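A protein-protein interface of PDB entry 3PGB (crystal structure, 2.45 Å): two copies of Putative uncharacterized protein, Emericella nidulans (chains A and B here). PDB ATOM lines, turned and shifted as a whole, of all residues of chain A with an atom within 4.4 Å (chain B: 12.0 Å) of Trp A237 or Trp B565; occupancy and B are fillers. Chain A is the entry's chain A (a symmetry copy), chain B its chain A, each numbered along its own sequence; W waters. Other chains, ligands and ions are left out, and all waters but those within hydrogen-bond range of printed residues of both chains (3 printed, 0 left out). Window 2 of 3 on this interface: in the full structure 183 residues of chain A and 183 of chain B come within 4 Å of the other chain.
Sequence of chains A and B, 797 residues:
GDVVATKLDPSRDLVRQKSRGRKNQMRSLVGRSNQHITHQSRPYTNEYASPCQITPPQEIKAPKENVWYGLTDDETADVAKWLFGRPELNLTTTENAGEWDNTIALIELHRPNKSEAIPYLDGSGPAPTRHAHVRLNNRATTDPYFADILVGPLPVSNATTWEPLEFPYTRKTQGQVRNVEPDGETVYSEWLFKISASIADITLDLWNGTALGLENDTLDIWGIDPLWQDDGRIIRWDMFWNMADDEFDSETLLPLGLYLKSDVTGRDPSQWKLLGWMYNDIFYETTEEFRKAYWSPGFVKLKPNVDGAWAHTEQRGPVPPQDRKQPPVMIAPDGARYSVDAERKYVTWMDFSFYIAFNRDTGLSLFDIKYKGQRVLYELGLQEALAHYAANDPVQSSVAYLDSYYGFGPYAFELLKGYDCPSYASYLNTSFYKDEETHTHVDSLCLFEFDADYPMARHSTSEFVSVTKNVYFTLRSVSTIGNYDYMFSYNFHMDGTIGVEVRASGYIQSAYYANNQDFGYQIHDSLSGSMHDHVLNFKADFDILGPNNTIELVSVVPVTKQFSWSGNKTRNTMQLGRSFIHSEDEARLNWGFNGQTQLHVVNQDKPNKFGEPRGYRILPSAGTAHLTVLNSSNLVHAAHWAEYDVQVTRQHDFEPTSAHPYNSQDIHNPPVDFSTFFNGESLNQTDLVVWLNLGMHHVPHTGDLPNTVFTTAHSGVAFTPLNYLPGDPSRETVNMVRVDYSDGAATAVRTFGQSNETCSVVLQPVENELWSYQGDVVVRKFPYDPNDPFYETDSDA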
ATOM      1  N   GLY A 223     -22.692  17.193 -24.791  1.00  0.00           N
ATOM      2  CA  GLY A 223     -21.348  16.719 -24.491  1.00  0.00           C
ATOM      3  C   GLY A 223     -20.284  17.768 -24.228  1.00  0.00           C
ATOM      4  O   GLY A 223     -20.340  18.489 -23.232  1.00  0.00           O
ATOM      5  N   ILE A 224     -19.317  17.852 -25.136  1.00  0.00           N
ATOM      6  CA  ILE A 224     -18.031  18.472 -24.831  1.00  0.00           C
ATOM      7  C   ILE A 224     -17.877  19.911 -25.311  1.00  0.00           C
ATOM      8  O   ILE A 224     -18.501  20.330 -26.286  1.00  0.00           O
ATOM      9  CB  ILE A 224     -16.852  17.618 -25.372  1.00  0.00           C
ATOM     10  CG1 ILE A 224     -16.824  17.606 -26.907  1.00  0.00           C
ATOM     11  CG2 ILE A 224     -16.950  16.216 -24.825  1.00  0.00           C
ATOM     12  CD1 ILE A 224     -15.664  16.833 -27.504  1.00  0.00           C
ATOM     13  N   TRP A 228     -13.432  18.277 -30.184  1.00  0.00           N
ATOM     14  CA  TRP A 228     -12.116  17.732 -30.528  1.00  0.00           C
ATOM     15  C   TRP A 228     -11.706  18.223 -31.903  1.00  0.00           C
ATOM     16  O   TRP A 228     -12.498  18.169 -32.845  1.00  0.00           O
ATOM     17  CB  TRP A 228     -12.130  16.203 -30.504  1.00  0.00           C
ATOM     18  CG  TRP A 228     -11.984  15.601 -29.131  1.00  0.00           C
ATOM     19  CD1 TRP A 228     -12.126  16.233 -27.934  1.00  0.00           C
ATOM     20  CD2 TRP A 228     -11.714  14.229 -28.829  1.00  0.00           C
ATOM     21  NE1 TRP A 228     -11.940  15.349 -26.907  1.00  0.00           N
ATOM     22  CE2 TRP A 228     -11.689  14.109 -27.427  1.00  0.00           C
ATOM     23  CE3 TRP A 228     -11.489  13.090 -29.609  1.00  0.00           C
ATOM     24  CZ2 TRP A 228     -11.439  12.900 -26.785  1.00  0.00           C
ATOM     25  CZ3 TRP A 228     -11.244  11.891 -28.971  1.00  0.00           C
ATOM     26  CH2 TRP A 228     -11.219  11.806 -27.571  1.00  0.00           C
ATOM     27  N   ILE A 235     -14.648  16.597 -34.009  1.00  0.00           N
ATOM     28  CA  ILE A 235     -15.227  15.399 -33.395  1.00  0.00           C
ATOM     29  C   ILE A 235     -15.976  15.716 -32.100  1.00  0.00           C
ATOM     30  O   ILE A 235     -15.540  16.542 -31.300  1.00  0.00           O
ATOM     31  CB  ILE A 235     -14.134  14.315 -33.137  1.00  0.00           C
ATOM     32  CG1 ILE A 235     -13.719  13.655 -34.461  1.00  0.00           C
ATOM     33  CG2 ILE A 235     -14.624  13.256 -32.166  1.00  0.00           C
ATOM     34  CD1 ILE A 235     -12.637  12.589 -34.317  1.00  0.00           C
ATOM     35  N   ARG A 236     -17.102  15.032 -31.919  1.00  0.00           N
ATOM     36  CA  ARG A 236     -17.985  15.190 -30.774  1.00  0.00           C
ATOM     37  C   ARG A 236     -17.947  13.937 -29.912  1.00  0.00           C
ATOM     38  O   ARG A 236     -17.822  12.833 -30.429  1.00  0.00           O
ATOM     39  CB  ARG A 236     -19.433  15.342 -31.245  1.00  0.00           C
ATOM     40  CG  ARG A 236     -19.939  16.753 -31.486  1.00  0.00           C
ATOM     41  CD  ARG A 236     -21.395  16.839 -31.064  1.00  0.00           C
ATOM     42  NE  ARG A 236     -21.922  18.191 -31.170  1.00  0.00           N
ATOM     43  CZ  ARG A 236     -22.865  18.708 -30.382  1.00  0.00           C
ATOM     44  NH1 ARG A 236     -23.413  18.000 -29.393  1.00  0.00           N
ATOM     45  NH2 ARG A 236     -23.258  19.962 -30.579  1.00  0.00           N
ATOM     46  N   TRP A 237     -18.071  14.123 -28.602  1.00  0.00           N
ATOM     47  CA  TRP A 237     -18.406  13.056 -27.663  1.00  0.00           C
ATOM     48  C   TRP A 237     -19.626  13.541 -26.889  1.00  0.00           C
ATOM     49  O   TRP A 237     -19.568  14.586 -26.239  1.00  0.00           O
ATOM     50  CB  TRP A 237     -17.259  12.807 -26.684  1.00  0.00           C
ATOM     51  CG  TRP A 237     -16.309  11.705 -27.065  1.00  0.00           C
ATOM     52  CD1 TRP A 237     -15.020  11.843 -27.492  1.00  0.00           C
ATOM     53  CD2 TRP A 237     -16.563  10.297 -27.012  1.00  0.00           C
ATOM     54  NE1 TRP A 237     -14.462  10.615 -27.717  1.00  0.00           N
ATOM     55  CE2 TRP A 237     -15.385   9.646 -27.431  1.00  0.00           C
ATOM     56  CE3 TRP A 237     -17.677   9.522 -26.661  1.00  0.00           C
ATOM     57  CZ2 TRP A 237     -15.286   8.256 -27.510  1.00  0.00           C
ATOM     58  CZ3 TRP A 237     -17.578   8.138 -26.742  1.00  0.00           C
ATOM     59  CH2 TRP A 237     -16.390   7.521 -27.162  1.00  0.00           C
ATOM     60  N   ASP A 238     -20.727  12.800 -26.959  1.00  0.00           N
ATOM     61  CA  ASP A 238     -21.961  13.199 -26.291  1.00  0.00           C
ATOM     62  C   ASP A 238     -22.460  12.124 -25.340  1.00  0.00           C
ATOM     63  O   ASP A 238     -22.093  10.955 -25.452  1.00  0.00           O
ATOM     64  CB  ASP A 238     -23.046  13.519 -27.316  1.00  0.00           C
ATOM     65  CG  ASP A 238     -22.676  14.684 -28.207  1.00  0.00           C
ATOM     66  OD1 ASP A 238     -22.660  15.827 -27.714  1.00  0.00           O
ATOM     67  OD2 ASP A 238     -22.405  14.456 -29.401  1.00  0.00           O
ATOM     68  N   TYR A 259     -22.245   6.969 -23.943  1.00  0.00           N
ATOM     69  CA  TYR A 259     -21.500   7.962 -24.709  1.00  0.00           C
ATOM     70  C   TYR A 259     -21.472   7.636 -26.198  1.00  0.00           C
ATOM     71  O   TYR A 259     -21.563   6.471 -26.593  1.00  0.00           O
ATOM     72  CB  TYR A 259     -20.086   8.083 -24.157  1.00  0.00           C
ATOM     73  CG  TYR A 259     -20.063   8.261 -22.655  1.00  0.00           C
ATOM     74  CD1 TYR A 259     -19.965   9.521 -22.082  1.00  0.00           C
ATOM     75  CD2 TYR A 259     -20.164   7.165 -21.809  1.00  0.00           C
ATOM     76  CE1 TYR A 259     -19.950   9.679 -20.712  1.00  0.00           C
ATOM     77  CE2 TYR A 259     -20.157   7.312 -20.438  1.00  0.00           C
ATOM     78  CZ  TYR A 259     -20.051   8.568 -19.896  1.00  0.00           C
ATOM     79  OH  TYR A 259     -20.036   8.697 -18.536  1.00  0.00           O
ATOM     80  N   LEU A 260     -21.346   8.684 -27.010  1.00  0.00           N
ATOM     81  CA  LEU A 260     -21.494   8.590 -28.460  1.00  0.00           C
ATOM     82  C   LEU A 260     -20.459   9.473 -29.138  1.00  0.00           C
ATOM     83  O   LEU A 260     -20.512  10.690 -29.003  1.00  0.00           O
ATOM     84  CB  LEU A 260     -22.900   9.044 -28.865  1.00  0.00           C
ATOM     85  CG  LEU A 260     -23.186   9.248 -30.357  1.00  0.00           C
ATOM     86  CD1 LEU A 260     -23.006   7.932 -31.118  1.00  0.00           C
ATOM     87  CD2 LEU A 260     -24.590   9.816 -30.562  1.00  0.00           C
ATOM     88  N   LYS A 261     -19.529   8.854 -29.863  1.00  0.00           N
ATOM     89  CA  LYS A 261     -18.498   9.587 -30.591  1.00  0.00           C
ATOM     90  C   LYS A 261     -18.952   9.832 -32.030  1.00  0.00           C
ATOM     91  O   LYS A 261     -19.452   8.921 -32.699  1.00  0.00           O
ATOM     92  CB  LYS A 261     -17.173   8.821 -30.561  1.00  0.00           C
ATOM     93  CG  LYS A 261     -15.941   9.671 -30.877  1.00  0.00           C
ATOM     94  CD  LYS A 261     -14.674   8.823 -30.931  1.00  0.00           C
ATOM     95  CE  LYS A 261     -13.416   9.672 -31.083  1.00  0.00           C
ATOM     96  NZ  LYS A 261     -12.174   8.837 -31.091  1.00  0.00           N
ATOM     97  N   MET A 278     -19.686   4.259 -25.901  1.00  0.00           N
ATOM     98  CA  MET A 278     -19.068   3.723 -24.672  1.00  0.00           C
ATOM     99  C   MET A 278     -20.108   3.559 -23.574  1.00  0.00           C
ATOM    100  O   MET A 278     -21.020   4.368 -23.449  1.00  0.00           O
ATOM    101  CB  MET A 278     -17.918   4.603 -24.174  1.00  0.00           C
ATOM    102  CG  MET A 278     -17.030   3.939 -23.105  1.00  0.00           C
ATOM    103  SD  MET A 278     -17.658   3.989 -21.396  1.00  0.00           S
ATOM    104  CE  MET A 278     -17.257   5.676 -20.950  1.00  0.00           C
ATOM    105  N   PHE A 283     -15.892  -0.126 -25.012  1.00  0.00           N
ATOM    106  CA  PHE A 283     -16.053   0.593 -26.274  1.00  0.00           C
ATOM    107  C   PHE A 283     -16.643  -0.308 -27.363  1.00  0.00           C
ATOM    108  O   PHE A 283     -16.260  -1.473 -27.487  1.00  0.00           O
ATOM    109  CB  PHE A 283     -14.697   1.127 -26.729  1.00  0.00           C
ATOM    110  CG  PHE A 283     -14.771   2.030 -27.928  1.00  0.00           C
ATOM    111  CD1 PHE A 283     -15.271   3.321 -27.812  1.00  0.00           C
ATOM    112  CD2 PHE A 283     -14.330   1.596 -29.174  1.00  0.00           C
ATOM    113  CE1 PHE A 283     -15.339   4.161 -28.918  1.00  0.00           C
ATOM    114  CE2 PHE A 283     -14.391   2.435 -30.288  1.00  0.00           C
ATOM    115  CZ  PHE A 283     -14.898   3.717 -30.156  1.00  0.00           C
ATOM    116  N   ASN A 392     -12.782   9.281 -16.159  1.00  0.00           N
ATOM    117  CA  ASN A 392     -12.563   8.046 -16.898  1.00  0.00           C
ATOM    118  C   ASN A 392     -13.540   7.908 -18.070  1.00  0.00           C
ATOM    119  O   ASN A 392     -13.495   6.917 -18.789  1.00  0.00           O
ATOM    120  CB  ASN A 392     -12.682   6.834 -15.965  1.00  0.00           C
ATOM    121  CG  ASN A 392     -11.990   5.591 -16.510  1.00  0.00           C
ATOM    122  OD1 ASN A 392     -11.118   5.675 -17.373  1.00  0.00           O
ATOM    123  ND2 ASN A 392     -12.368   4.430 -15.992  1.00  0.00           N
ATOM    124  N   ASP A 393     -14.422   8.891 -18.258  1.00  0.00           N
ATOM    125  CA  ASP A 393     -15.335   8.914 -19.398  1.00  0.00           C
ATOM    126  C   ASP A 393     -14.932  10.047 -20.348  1.00  0.00           C
ATOM    127  O   ASP A 393     -14.297  10.999 -19.920  1.00  0.00           O
ATOM    128  CB  ASP A 393     -16.795   9.018 -18.928  1.00  0.00           C
ATOM    129  CG  ASP A 393     -17.204  10.427 -18.501  1.00  0.00           C
ATOM    130  OD1 ASP A 393     -17.124  11.365 -19.327  1.00  0.00           O
ATOM    131  OD2 ASP A 393     -17.665  10.582 -17.347  1.00  0.00           O
ATOM    132  N   PRO A 394     -15.283   9.939 -21.642  1.00  0.00           N
ATOM    133  CA  PRO A 394     -14.774  10.881 -22.638  1.00  0.00           C
ATOM    134  C   PRO A 394     -15.401  12.272 -22.608  1.00  0.00           C
ATOM    135  O   PRO A 394     -14.764  13.235 -23.030  1.00  0.00           O
ATOM    136  CB  PRO A 394     -15.129  10.204 -23.961  1.00  0.00           C
ATOM    137  CG  PRO A 394     -16.355   9.421 -23.659  1.00  0.00           C
ATOM    138  CD  PRO A 394     -16.220   8.966 -22.236  1.00  0.00           C
ATOM    139  N   VAL A 395     -16.642  12.378 -22.150  1.00  0.00           N
ATOM    140  CA  VAL A 395     -17.303  13.674 -22.095  1.00  0.00           C
ATOM    141  C   VAL A 395     -16.666  14.540 -21.006  1.00  0.00           C
ATOM    142  O   VAL A 395     -16.162  15.637 -21.285  1.00  0.00           O
ATOM    143  CB  VAL A 395     -18.824  13.529 -21.879  1.00  0.00           C
ATOM    144  CG1 VAL A 395     -19.436  14.838 -21.357  1.00  0.00           C
ATOM    145  CG2 VAL A 395     -19.499  13.086 -23.185  1.00  0.00           C
ATOM    146  N   SER A 397     -13.916  13.934 -19.388  1.00  0.00           N
ATOM    147  CA  SER A 397     -12.478  14.037 -19.660  1.00  0.00           C
ATOM    148  C   SER A 397     -12.155  15.209 -20.589  1.00  0.00           C
ATOM    149  O   SER A 397     -11.113  15.838 -20.462  1.00  0.00           O
ATOM    150  CB  SER A 397     -11.942  12.734 -20.263  1.00  0.00           C
ATOM    151  OG  SER A 397     -10.565  12.838 -20.583  1.00  0.00           O
ATOM    152  N   VAL B 559      -1.510  13.567 -15.207  1.00  0.00           N
ATOM    153  CA  VAL B 559      -1.203  12.268 -15.795  1.00  0.00           C
ATOM    154  C   VAL B 559      -1.444  12.332 -17.288  1.00  0.00           C
ATOM    155  O   VAL B 559      -2.356  13.035 -17.750  1.00  0.00           O
ATOM    156  CB  VAL B 559      -2.104  11.128 -15.237  1.00  0.00           C
ATOM    157  CG1 VAL B 559      -1.633  10.680 -13.870  1.00  0.00           C
ATOM    158  CG2 VAL B 559      -3.561  11.560 -15.192  1.00  0.00           C
ATOM    159  N   THR B 560      -0.617  11.608 -18.039  1.00  0.00           N
ATOM    160  CA  THR B 560      -0.951  11.227 -19.406  1.00  0.00           C
ATOM    161  C   THR B 560      -1.492   9.804 -19.335  1.00  0.00           C
ATOM    162  O   THR B 560      -0.851   8.915 -18.779  1.00  0.00           O
ATOM    163  CB  THR B 560       0.249  11.326 -20.336  1.00  0.00           C
ATOM    164  OG1 THR B 560       0.724  12.676 -20.315  1.00  0.00           O
ATOM    165  N   LYS B 561      -2.683   9.607 -19.887  1.00  0.00           N
ATOM    166  CA  LYS B 561      -3.472   8.415 -19.616  1.00  0.00           C
ATOM    167  C   LYS B 561      -4.045   7.854 -20.906  1.00  0.00           C
ATOM    168  O   LYS B 561      -4.393   8.596 -21.824  1.00  0.00           O
ATOM    169  CB  LYS B 561      -4.620   8.790 -18.670  1.00  0.00           C
ATOM    170  CG  LYS B 561      -5.361   7.618 -18.012  1.00  0.00           C
ATOM    171  CD  LYS B 561      -4.921   7.383 -16.571  1.00  0.00           C
ATOM    172  CE  LYS B 561      -5.922   6.505 -15.822  1.00  0.00           C
ATOM    173  NZ  LYS B 561      -6.344   5.294 -16.593  1.00  0.00           N
ATOM    174  N   GLN B 562      -4.137   6.534 -20.965  1.00  0.00           N
ATOM    175  CA  GLN B 562      -4.856   5.847 -22.025  1.00  0.00           C
ATOM    176  C   GLN B 562      -6.200   5.378 -21.461  1.00  0.00           C
ATOM    177  O   GLN B 562      -6.325   5.125 -20.258  1.00  0.00           O
ATOM    178  CB  GLN B 562      -4.028   4.661 -22.506  1.00  0.00           C
ATOM    179  CG  GLN B 562      -4.521   4.004 -23.781  1.00  0.00           C
ATOM    180  CD  GLN B 562      -3.685   2.796 -24.170  1.00  0.00           C
ATOM    181  OE1 GLN B 562      -2.717   2.445 -23.487  1.00  0.00           O
ATOM    182  NE2 GLN B 562      -4.063   2.147 -25.260  1.00  0.00           N
ATOM    183  N   PHE B 563      -7.196   5.272 -22.330  1.00  0.00           N
ATOM    184  CA  PHE B 563      -8.546   4.884 -21.934  1.00  0.00           C
ATOM    185  C   PHE B 563      -9.118   3.840 -22.882  1.00  0.00           C
ATOM    186  O   PHE B 563      -8.642   3.684 -24.008  1.00  0.00           O
ATOM    187  CB  PHE B 563      -9.480   6.096 -21.938  1.00  0.00           C
ATOM    188  CG  PHE B 563      -9.027   7.223 -21.066  1.00  0.00           C
ATOM    189  CD1 PHE B 563      -8.213   8.226 -21.572  1.00  0.00           C
ATOM    190  CD2 PHE B 563      -9.432   7.295 -19.741  1.00  0.00           C
ATOM    191  CE1 PHE B 563      -7.798   9.273 -20.767  1.00  0.00           C
ATOM    192  CE2 PHE B 563      -9.024   8.343 -18.930  1.00  0.00           C
ATOM    193  CZ  PHE B 563      -8.209   9.333 -19.445  1.00  0.00           C
ATOM    194  N   SER B 564     -10.172   3.159 -22.430  1.00  0.00           N
ATOM    195  CA  SER B 564     -10.884   2.175 -23.253  1.00  0.00           C
ATOM    196  C   SER B 564     -11.529   2.788 -24.501  1.00  0.00           C
ATOM    197  O   SER B 564     -11.807   2.082 -25.471  1.00  0.00           O
ATOM    198  CB  SER B 564     -11.960   1.469 -22.422  1.00  0.00           C
ATOM    199  OG  SER B 564     -12.906   2.395 -21.918  1.00  0.00           O
ATOM    200  N   TRP B 565     -11.744   4.101 -24.464  1.00  0.00           N
ATOM    201  CA  TRP B 565     -12.390   4.844 -25.547  1.00  0.00           C
ATOM    202  C   TRP B 565     -11.389   5.721 -26.304  1.00  0.00           C
ATOM    203  O   TRP B 565     -11.773   6.516 -27.162  1.00  0.00           O
ATOM    204  CB  TRP B 565     -13.517   5.713 -24.970  1.00  0.00           C
ATOM    205  CG  TRP B 565     -13.142   6.423 -23.682  1.00  0.00           C
ATOM    206  CD1 TRP B 565     -13.403   6.000 -22.410  1.00  0.00           C
ATOM    207  CD2 TRP B 565     -12.432   7.660 -23.553  1.00  0.00           C
ATOM    208  NE1 TRP B 565     -12.910   6.898 -21.500  1.00  0.00           N
ATOM    209  CE2 TRP B 565     -12.309   7.929 -22.173  1.00  0.00           C
ATOM    210  CE3 TRP B 565     -11.889   8.569 -24.469  1.00  0.00           C
ATOM    211  CZ2 TRP B 565     -11.663   9.065 -21.684  1.00  0.00           C
ATOM    212  CZ3 TRP B 565     -11.247   9.704 -23.980  1.00  0.00           C
ATOM    213  CH2 TRP B 565     -11.141   9.941 -22.600  1.00  0.00           C
ATOM    214  N   SER B 566     -10.107   5.545 -25.999  1.00  0.00           N
ATOM    215  CA  SER B 566      -9.040   6.423 -26.481  1.00  0.00           C
ATOM    216  C   SER B 566      -8.444   5.964 -27.814  1.00  0.00           C
ATOM    217  O   SER B 566      -7.920   6.775 -28.582  1.00  0.00           O
ATOM    218  CB  SER B 566      -7.937   6.485 -25.428  1.00  0.00           C
ATOM    219  OG  SER B 566      -7.059   7.555 -25.677  1.00  0.00           O
ATOM    220  N   GLY B 567      -8.508   4.659 -28.072  1.00  0.00           N
ATOM    221  CA  GLY B 567      -8.087   4.098 -29.355  1.00  0.00           C
ATOM    222  C   GLY B 567      -6.584   4.151 -29.573  1.00  0.00           C
ATOM    223  O   GLY B 567      -6.115   4.582 -30.637  1.00  0.00           O
ATOM    224  N   ASN B 568      -5.827   3.720 -28.566  1.00  0.00           N
ATOM    225  CA  ASN B 568      -4.362   3.748 -28.634  1.00  0.00           C
ATOM    226  C   ASN B 568      -3.779   5.161 -28.568  1.00  0.00           C
ATOM    227  O   ASN B 568      -2.568   5.333 -28.716  1.00  0.00           O
ATOM    228  CB  ASN B 568      -3.850   3.037 -29.900  1.00  0.00           C
ATOM    229  N   LYS B 569      -4.634   6.161 -28.342  1.00  0.00           N
ATOM    230  CA  LYS B 569      -4.183   7.530 -28.106  1.00  0.00           C
ATOM    231  C   LYS B 569      -4.145   7.794 -26.600  1.00  0.00           C
ATOM    232  O   LYS B 569      -4.840   7.129 -25.832  1.00  0.00           O
ATOM    233  CB  LYS B 569      -5.114   8.534 -28.790  1.00  0.00           C
ATOM    234  CG  LYS B 569      -5.067   8.525 -30.322  1.00  0.00           C
ATOM    235  CD  LYS B 569      -5.896   9.685 -30.900  1.00  0.00           C
ATOM    236  CE  LYS B 569      -5.416  10.124 -32.287  1.00  0.00           C
ATOM    237  NZ  LYS B 569      -5.883  11.513 -32.648  1.00  0.00           N
ATOM    238  N   THR B 570      -3.320   8.751 -26.185  1.00  0.00           N
ATOM    239  CA  THR B 570      -3.292   9.187 -24.787  1.00  0.00           C
ATOM    240  C   THR B 570      -3.679  10.661 -24.684  1.00  0.00           C
ATOM    241  O   THR B 570      -3.581  11.419 -25.652  1.00  0.00           O
ATOM    242  CB  THR B 570      -1.910   8.959 -24.118  1.00  0.00           C
ATOM    243  OG1 THR B 570      -0.934   9.830 -24.694  1.00  0.00           O
ATOM    244  CG2 THR B 570      -1.458   7.521 -24.288  1.00  0.00           C
ATOM    245  N   ARG B 571      -4.135  11.051 -23.502  1.00  0.00           N
ATOM    246  CA  ARG B 571      -4.545  12.425 -23.261  1.00  0.00           C
ATOM    247  C   ARG B 571      -3.882  12.975 -22.014  1.00  0.00           C
ATOM    248  O   ARG B 571      -3.747  12.280 -21.009  1.00  0.00           O
ATOM    249  CB  ARG B 571      -6.065  12.515 -23.148  1.00  0.00           C
ATOM    250  CG  ARG B 571      -6.753  12.333 -24.487  1.00  0.00           C
ATOM    251  CD  ARG B 571      -8.172  12.859 -24.501  1.00  0.00           C
ATOM    252  NE  ARG B 571      -8.455  13.467 -25.802  1.00  0.00           N
ATOM    253  CZ  ARG B 571      -8.561  14.775 -26.047  1.00  0.00           C
ATOM    254  NH1 ARG B 571      -8.437  15.678 -25.079  1.00  0.00           N
ATOM    255  NH2 ARG B 571      -8.812  15.185 -27.289  1.00  0.00           N
ATOM    256  N   ASN B 572      -3.453  14.227 -22.099  1.00  0.00           N
ATOM    257  CA  ASN B 572      -2.876  14.916 -20.964  1.00  0.00           C
ATOM    258  C   ASN B 572      -4.012  15.485 -20.122  1.00  0.00           C
ATOM    259  O   ASN B 572      -4.719  16.405 -20.539  1.00  0.00           O
ATOM    260  CB  ASN B 572      -1.918  16.003 -21.436  1.00  0.00           C
ATOM    261  CG  ASN B 572      -0.801  15.453 -22.316  1.00  0.00           C
ATOM    262  OD1 ASN B 572      -0.395  14.295 -22.176  1.00  0.00           O
ATOM    263  ND2 ASN B 572      -0.307  16.277 -23.232  1.00  0.00           N
ATOM    264  N   THR B 573      -4.179  14.901 -18.938  1.00  0.00           N
ATOM    265  CA  THR B 573      -5.336  15.134 -18.091  1.00  0.00           C
ATOM    266  C   THR B 573      -4.862  15.225 -16.643  1.00  0.00           C
ATOM    267  O   THR B 573      -3.753  15.683 -16.389  1.00  0.00           O
ATOM    268  CB  THR B 573      -6.390  14.004 -18.301  1.00  0.00           C
ATOM    269  OG1 THR B 573      -7.499  14.186 -17.414  1.00  0.00           O
ATOM    270  CG2 THR B 573      -5.781  12.634 -18.068  1.00  0.00           C
ATOM    271  N   MET B 574      -5.708  14.828 -15.699  1.00  0.00           N
ATOM    272  CA  MET B 574      -5.340  14.776 -14.287  1.00  0.00           C
ATOM    273  C   MET B 574      -6.168  13.713 -13.587  1.00  0.00           C
ATOM    274  O   MET B 574      -7.102  13.171 -14.162  1.00  0.00           O
ATOM    275  CB  MET B 574      -5.515  16.144 -13.609  1.00  0.00           C
ATOM    276  CG  MET B 574      -6.948  16.677 -13.552  1.00  0.00           C
ATOM    277  SD  MET B 574      -7.024  18.333 -12.822  1.00  0.00           S
ATOM    278  CE  MET B 574      -8.734  18.793 -13.088  1.00  0.00           C
ATOM    279  N   GLN B 575      -5.831  13.442 -12.333  1.00  0.00           N
ATOM    280  CA  GLN B 575      -6.324  12.269 -11.629  1.00  0.00           C
ATOM    281  C   GLN B 575      -6.293  12.521 -10.125  1.00  0.00           C
ATOM    282  O   GLN B 575      -5.582  13.415  -9.653  1.00  0.00           O
ATOM    283  CB  GLN B 575      -5.410  11.098 -11.978  1.00  0.00           C
ATOM    284  CG  GLN B 575      -5.864   9.733 -11.538  1.00  0.00           C
ATOM    285  CD  GLN B 575      -4.819   8.670 -11.833  1.00  0.00           C
ATOM    286  OE1 GLN B 575      -4.307   8.017 -10.918  1.00  0.00           O
ATOM    287  NE2 GLN B 575      -4.491   8.498 -13.114  1.00  0.00           N
HETATM  288  O   HOH W   1     -11.122   3.653 -19.336  1.00  0.00           O
HETATM  289  O   HOH W   2     -11.660   5.779 -30.089  1.00  0.00           O
HETATM  290  O   HOH W   3      -9.510  12.656 -18.259  1.00  0.00           O
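Trp B565 touches Trp A237. Ser B564 touches Phe A283. Phe A283 touches Trp B565 (CD1 to CA, 3.97 Å). Phe B563 touches Asn A392 (CD2 to OD1, 3.3 Å). Asp A393 touches Trp B565. Pro A394 touches Trp B565. CH2 of Trp B565 touches OG of Ser A397 (3.6 Å).
Of chain B, only Trp B565 comes within 4 Å of Trp A237. Gly A223 touches none of the printed residues of chain B. No residue of chain B comes within 4 Å of Ile A224. No residue of chain B comes within 4 Å of Ile A235. No residue of chain B comes within 4 Å of Leu A260. No residue of chain B comes within 4 Å of Lys A261. Of the printed residues of chain B, Phe A283 touches Ser B564 and Trp B565. Asn A392 touches just these residues of chain B: Phe B563 (3.3 Å) and Trp B565 (2.8 Å). No residue of chain B comes within 4 Å of Val A395. Of the printed residues of chain A, Phe B563 touches Asn A392 (3.3 Å). Of the printed residues of chain A, Arg B571 touches Trp A228 (3.1 Å). The nearest residue of chain B that does not touch Trp A237 is Ser B566 (6.0 Å).
Of the 17 printed residues of chain B, 4 touch a printed residue of chain A. Hydrophobic or aromatic side chains of chain B within 4 Å of the printed part of chain A: Phe B563 and Trp B565. Among the printed residues, no Asp or Glu carboxylate lies within 4 Å of a Lys or Arg side-chain nitrogen of the other chain.
Water W3 bridges the side-chain hydroxyl of Ser A397 (2.6 Å) and the side-chain hydroxyl of Thr B573 (2.7 Å). Water W1 bridges OD1 of Asn A392 (2.8 Å) and N of Ser B564 (3.3 Å). Water W2 bridges the backbone carbonyl oxygen (O) of Trp B565 (3.0 Å) and the side-chain amino group (NZ) of Lys A261 (3.3 Å).
NH2 of Arg B571 lies close to NE1 of Trp A228. O of Asn A392 sits at hydrogen-bond distance from NE1 of Trp B565 (2.8 Å).
The side-chain carboxylate of Asp A393 is in hydrogen-bond range of the backbone NH of Val A395 (3.0 Å). The backbone carbonyl oxygen (O) of Trp A228 is in hydrogen-bond range of the backbone NH (N) of Ile A235 (2.9 Å). The backbone NH (N) of Arg B571 lies within hydrogen-bond range of the backbone carbonyl oxygen (O) of Lys B561, at 3.0 Å. The side-chain hydroxyl (OH) of Tyr A259 is in hydrogen-bond range of the side-chain carboxylate (OD2) of Asp A393, 3.3 Å away. N of Ile A224 lies close to O of Trp A237 (3.5 Å).
No position is printed for both chains. Of the 9 pairs that touch across the chains among the printed residues, none has its exchanged pair printed and touching as well.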
